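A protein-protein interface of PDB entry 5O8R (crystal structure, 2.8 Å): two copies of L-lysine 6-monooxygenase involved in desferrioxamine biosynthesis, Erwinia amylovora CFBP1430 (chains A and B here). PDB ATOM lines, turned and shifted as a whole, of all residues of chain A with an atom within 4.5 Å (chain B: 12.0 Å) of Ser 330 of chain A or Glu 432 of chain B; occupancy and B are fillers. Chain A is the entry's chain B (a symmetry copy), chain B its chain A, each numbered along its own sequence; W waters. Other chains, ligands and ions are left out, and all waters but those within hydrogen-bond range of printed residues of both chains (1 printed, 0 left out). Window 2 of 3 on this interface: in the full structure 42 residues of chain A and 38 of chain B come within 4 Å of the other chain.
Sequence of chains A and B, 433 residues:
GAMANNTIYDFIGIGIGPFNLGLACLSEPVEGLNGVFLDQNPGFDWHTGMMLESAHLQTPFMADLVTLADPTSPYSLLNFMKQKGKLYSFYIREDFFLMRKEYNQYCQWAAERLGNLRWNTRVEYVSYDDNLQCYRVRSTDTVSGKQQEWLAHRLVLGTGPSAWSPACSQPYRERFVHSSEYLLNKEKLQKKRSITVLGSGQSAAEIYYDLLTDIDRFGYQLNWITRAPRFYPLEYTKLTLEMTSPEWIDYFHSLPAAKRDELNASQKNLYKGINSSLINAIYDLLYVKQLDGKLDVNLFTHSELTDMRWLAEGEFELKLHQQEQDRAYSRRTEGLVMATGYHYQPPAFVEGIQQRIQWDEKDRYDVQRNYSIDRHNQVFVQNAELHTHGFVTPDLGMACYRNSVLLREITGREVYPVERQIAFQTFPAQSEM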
ATOM      1  N   GLN A 221     -17.390 -17.330 -24.967  1.00  0.00           N
ATOM      2  CA  GLN A 221     -17.225 -16.286 -23.994  1.00  0.00           C
ATOM      3  C   GLN A 221     -17.747 -15.040 -24.667  1.00  0.00           C
ATOM      4  O   GLN A 221     -17.455 -14.808 -25.844  1.00  0.00           O
ATOM      5  CB  GLN A 221     -15.751 -16.124 -23.647  1.00  0.00           C
ATOM      6  CG  GLN A 221     -15.514 -15.173 -22.522  1.00  0.00           C
ATOM      7  CD  GLN A 221     -14.068 -15.042 -22.182  1.00  0.00           C
ATOM      8  OE1 GLN A 221     -13.650 -15.400 -21.088  1.00  0.00           O
ATOM      9  NE2 GLN A 221     -13.294 -14.492 -23.102  1.00  0.00           N
ATOM     10  N   GLU A 317      -5.512  -9.256 -29.794  1.00  0.00           N
ATOM     11  CA  GLU A 317      -5.148  -8.772 -28.496  1.00  0.00           C
ATOM     12  C   GLU A 317      -5.464  -7.284 -28.509  1.00  0.00           C
ATOM     13  O   GLU A 317      -4.957  -6.538 -29.334  1.00  0.00           O
ATOM     14  CB  GLU A 317      -3.681  -9.080 -28.218  1.00  0.00           C
ATOM     15  CG  GLU A 317      -3.230  -8.890 -26.780  1.00  0.00           C
ATOM     16  CD  GLU A 317      -1.995  -7.987 -26.643  1.00  0.00           C
ATOM     17  OE1 GLU A 317      -1.085  -8.431 -25.920  1.00  0.00           O
ATOM     18  OE2 GLU A 317      -1.924  -6.843 -27.215  1.00  0.00           O
ATOM     19  N   LEU A 318      -6.341  -6.861 -27.608  1.00  0.00           N
ATOM     20  CA  LEU A 318      -6.871  -5.509 -27.628  1.00  0.00           C
ATOM     21  C   LEU A 318      -6.184  -4.766 -26.526  1.00  0.00           C
ATOM     22  O   LEU A 318      -6.367  -5.105 -25.359  1.00  0.00           O
ATOM     23  CB  LEU A 318      -8.391  -5.512 -27.379  1.00  0.00           C
ATOM     24  CG  LEU A 318      -9.272  -6.448 -28.203  1.00  0.00           C
ATOM     25  CD1 LEU A 318     -10.634  -6.644 -27.576  1.00  0.00           C
ATOM     26  CD2 LEU A 318      -9.450  -5.932 -29.602  1.00  0.00           C
ATOM     27  N   TYR A 329      -4.175  -1.910 -20.218  1.00  0.00           N
ATOM     28  CA  TYR A 329      -4.379  -3.347 -20.018  1.00  0.00           C
ATOM     29  C   TYR A 329      -4.734  -3.969 -21.334  1.00  0.00           C
ATOM     30  O   TYR A 329      -5.051  -3.286 -22.326  1.00  0.00           O
ATOM     31  CB  TYR A 329      -5.458  -3.702 -18.949  1.00  0.00           C
ATOM     32  CG  TYR A 329      -6.941  -3.358 -19.252  1.00  0.00           C
ATOM     33  CD1 TYR A 329      -7.429  -2.056 -19.134  1.00  0.00           C
ATOM     34  CD2 TYR A 329      -7.854  -4.346 -19.609  1.00  0.00           C
ATOM     35  CE1 TYR A 329      -8.770  -1.759 -19.382  1.00  0.00           C
ATOM     36  CE2 TYR A 329      -9.190  -4.053 -19.854  1.00  0.00           C
ATOM     37  CZ  TYR A 329      -9.629  -2.768 -19.746  1.00  0.00           C
ATOM     38  OH  TYR A 329     -10.923  -2.523 -19.995  1.00  0.00           O
ATOM     39  N   SER A 330      -4.682  -5.284 -21.320  1.00  0.00           N
ATOM     40  CA  SER A 330      -4.730  -6.045 -22.514  1.00  0.00           C
ATOM     41  C   SER A 330      -5.754  -7.172 -22.301  1.00  0.00           C
ATOM     42  O   SER A 330      -5.860  -7.740 -21.201  1.00  0.00           O
ATOM     43  CB  SER A 330      -3.295  -6.512 -22.813  1.00  0.00           C
ATOM     44  OG  SER A 330      -3.253  -7.742 -23.511  1.00  0.00           O
ATOM     45  N   ARG A 331      -6.509  -7.465 -23.353  1.00  0.00           N
ATOM     46  CA  ARG A 331      -7.616  -8.403 -23.308  1.00  0.00           C
ATOM     47  C   ARG A 331      -7.615  -9.119 -24.668  1.00  0.00           C
ATOM     48  O   ARG A 331      -7.131  -8.536 -25.641  1.00  0.00           O
ATOM     49  CB  ARG A 331      -8.884  -7.554 -23.108  1.00  0.00           C
ATOM     50  CG  ARG A 331     -10.062  -8.249 -22.459  1.00  0.00           C
ATOM     51  CD  ARG A 331      -9.909  -8.258 -20.951  1.00  0.00           C
ATOM     52  NE  ARG A 331     -10.410  -9.533 -20.451  1.00  0.00           N
ATOM     53  CZ  ARG A 331     -10.209  -9.975 -19.226  1.00  0.00           C
ATOM     54  NH1 ARG A 331      -9.524  -9.224 -18.345  1.00  0.00           N
ATOM     55  NH2 ARG A 331     -10.702 -11.171 -18.884  1.00  0.00           N
ATOM     56  N   ARG A 332      -8.148 -10.332 -24.789  1.00  0.00           N
ATOM     57  CA  ARG A 332      -8.104 -11.017 -26.094  1.00  0.00           C
ATOM     58  C   ARG A 332      -9.383 -11.719 -26.439  1.00  0.00           C
ATOM     59  O   ARG A 332     -10.087 -12.135 -25.542  1.00  0.00           O
ATOM     60  CB  ARG A 332      -6.971 -12.048 -26.128  1.00  0.00           C
ATOM     61  CG  ARG A 332      -7.136 -13.262 -25.196  1.00  0.00           C
ATOM     62  CD  ARG A 332      -5.899 -14.160 -25.160  1.00  0.00           C
ATOM     63  NE  ARG A 332      -4.682 -13.350 -25.223  1.00  0.00           N
ATOM     64  CZ  ARG A 332      -3.567 -13.658 -25.876  1.00  0.00           C
ATOM     65  NH1 ARG A 332      -3.437 -14.809 -26.545  1.00  0.00           N
ATOM     66  NH2 ARG A 332      -2.557 -12.789 -25.851  1.00  0.00           N
ATOM     67  N   THR B 426     -16.539  -6.138 -14.414  1.00  0.00           N
ATOM     68  CA  THR B 426     -15.289  -5.781 -13.748  1.00  0.00           C
ATOM     69  C   THR B 426     -15.064  -4.267 -13.842  1.00  0.00           C
ATOM     70  O   THR B 426     -15.183  -3.670 -14.931  1.00  0.00           O
ATOM     71  CB  THR B 426     -14.122  -6.509 -14.390  1.00  0.00           C
ATOM     72  OG1 THR B 426     -14.459  -7.892 -14.504  1.00  0.00           O
ATOM     73  CG2 THR B 426     -12.863  -6.352 -13.564  1.00  0.00           C
ATOM     74  N   PRO B 428     -12.148  -2.200 -12.389  1.00  0.00           N
ATOM     75  CA  PRO B 428     -10.808  -1.692 -12.694  1.00  0.00           C
ATOM     76  C   PRO B 428     -10.306  -2.292 -13.981  1.00  0.00           C
ATOM     77  O   PRO B 428     -10.866  -3.273 -14.492  1.00  0.00           O
ATOM     78  CB  PRO B 428      -9.972  -2.236 -11.549  1.00  0.00           C
ATOM     79  CG  PRO B 428     -10.599  -3.575 -11.279  1.00  0.00           C
ATOM     80  CD  PRO B 428     -12.083  -3.364 -11.474  1.00  0.00           C
ATOM     81  N   ALA B 429      -9.227  -1.731 -14.486  1.00  0.00           N
ATOM     82  CA  ALA B 429      -8.509  -2.388 -15.540  1.00  0.00           C
ATOM     83  C   ALA B 429      -8.100  -3.743 -15.013  1.00  0.00           C
ATOM     84  O   ALA B 429      -7.971  -3.920 -13.820  1.00  0.00           O
ATOM     85  CB  ALA B 429      -7.300  -1.575 -15.933  1.00  0.00           C
ATOM     86  N   GLN B 430      -7.961  -4.706 -15.909  1.00  0.00           N
ATOM     87  CA  GLN B 430      -7.595  -6.077 -15.559  1.00  0.00           C
ATOM     88  C   GLN B 430      -7.173  -6.745 -16.845  1.00  0.00           C
ATOM     89  O   GLN B 430      -7.848  -6.596 -17.848  1.00  0.00           O
ATOM     90  CB  GLN B 430      -8.783  -6.835 -14.979  1.00  0.00           C
ATOM     91  CG  GLN B 430      -8.581  -8.351 -14.924  1.00  0.00           C
ATOM     92  CD  GLN B 430      -9.705  -9.072 -14.209  1.00  0.00           C
ATOM     93  OE1 GLN B 430     -10.101  -8.653 -13.116  1.00  0.00           O
ATOM     94  NE2 GLN B 430     -10.216 -10.171 -14.810  1.00  0.00           N
ATOM     95  N   SER B 431      -6.088  -7.508 -16.815  1.00  0.00           N
ATOM     96  CA  SER B 431      -5.473  -8.012 -18.053  1.00  0.00           C
ATOM     97  C   SER B 431      -5.754  -9.513 -18.165  1.00  0.00           C
ATOM     98  O   SER B 431      -6.174 -10.128 -17.180  1.00  0.00           O
ATOM     99  CB  SER B 431      -3.968  -7.697 -18.061  1.00  0.00           C
ATOM    100  OG  SER B 431      -3.704  -6.424 -17.487  1.00  0.00           O
ATOM    101  N   GLU B 432      -5.525 -10.095 -19.348  1.00  0.00           N
ATOM    102  CA  GLU B 432      -5.798 -11.521 -19.614  1.00  0.00           C
ATOM    103  C   GLU B 432      -4.559 -12.198 -20.237  1.00  0.00           C
ATOM    104  O   GLU B 432      -3.634 -12.611 -19.535  1.00  0.00           O
ATOM    105  CB  GLU B 432      -7.001 -11.606 -20.557  1.00  0.00           C
ATOM    106  CG  GLU B 432      -7.619 -12.982 -20.765  1.00  0.00           C
ATOM    107  CD  GLU B 432      -8.597 -13.031 -21.961  1.00  0.00           C
ATOM    108  OE1 GLU B 432      -9.172 -14.124 -22.234  1.00  0.00           O
ATOM    109  OE2 GLU B 432      -8.792 -11.982 -22.647  1.00  0.00           O
HETATM  110  O   HOH W   1     -11.956 -12.235 -22.047  1.00  0.00           O
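The guanidinium group (NH1) of Arg 331 of chain A sits at hydrogen-bond distance from the backbone carbonyl oxygen (O) of Gln 430 of chain B, at 3.2 Å. OE2 of Glu 432 of chain B lies within salt-bridge range of NE of Arg 331 of chain A. The backbone NH (N) of Glu 432 of chain B lies within hydrogen-bond range of the backbone carbonyl oxygen (O) of Ser 330 of chain A (3.0 Å). The backbone NH (N) of Arg 332 of chain A lies within hydrogen-bond range of the side-chain carboxylate (OE2) of Glu 432 of chain B, at 2.8 Å.
The side-chain carboxylate (OE1) of Glu 317 of chain A sits at hydrogen-bond distance from the side-chain hydroxyl (OG) of Ser 330 of chain A (3.3 Å). The backbone carbonyl oxygen of Arg 331 of chain A lies within hydrogen-bond range of the backbone NH of Leu 318 of chain A (2.7 Å).
Among the printed residues, pairs that only touch across the chains: Tyr 329 of chain A with Gln 430 of chain B (2.9 Å), Ser 330 of chain A with Ser 431 of chain B (3.2 Å), Tyr 329 of chain A with Ala 429 of chain B (3.2 Å), Tyr 329 of chain A with Ser 431 of chain B (3.6 Å) and Arg 331 of chain A with Ser 431 of chain B (3.7 Å).
Of chain B, only Ala 429, Gln 430 and Ser 431 come within 4 Å of Tyr 329 of chain A. Arg 331 of chain A touches three residues of chain B. Of chain B, only Glu 432 (2.8 Å) comes within 4 Å of Arg 332 of chain A. Of the printed residues of chain A, Ala 429 of chain B touches Tyr 329. Printed residues of chain A within 4 Å of Gln 430 of chain B: Tyr 329 and Arg 331. Of the printed residues of chain A, Ser 431 of chain B touches Tyr 329, Ser 330 and Arg 331. Glu 432 of chain B touches just these residues of chain A: Ser 330 (3.0 Å), Arg 331 (3.7 Å) and Arg 332 (2.8 Å). The nearest printed residue of chain A that does not touch Ala 429 of chain B is Arg 331 of chain A (6.6 Å).
Of the 7 printed residues of chain A, 4 touch a printed residue of chain B. Printed residues of chain A that touch a printed residue of chain B: Tyr 329, Ser 330, Arg 331 and Arg 332. Hydrophobic or aromatic side chains of chain A that line the printed part of chain B: Tyr 329. Hydrophobic or aromatic side chains of chain B that line the printed part of chain A: Ala 429. Along chain B the printed residues that touch a printed residue of chain A span positions 429 to 432. Among the printed residues, 9 pairs touch across the chains. Among the printed residues, Asp or Glu carboxylates within 4 Å of a Lys or Arg side-chain nitrogen of the other chain: Arg 331 of chain A with Glu 432 of chain B.
No position is printed for both chains. Of the 9 pairs that touch across the chains among the printed residues, none has its exchanged pair printed and touching as well.
Water W1 lies within hydrogen-bond range of NE2 of Gln 221 of chain A, OE2 of Glu 432 of chain B and NE of Arg 331 of chain A.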
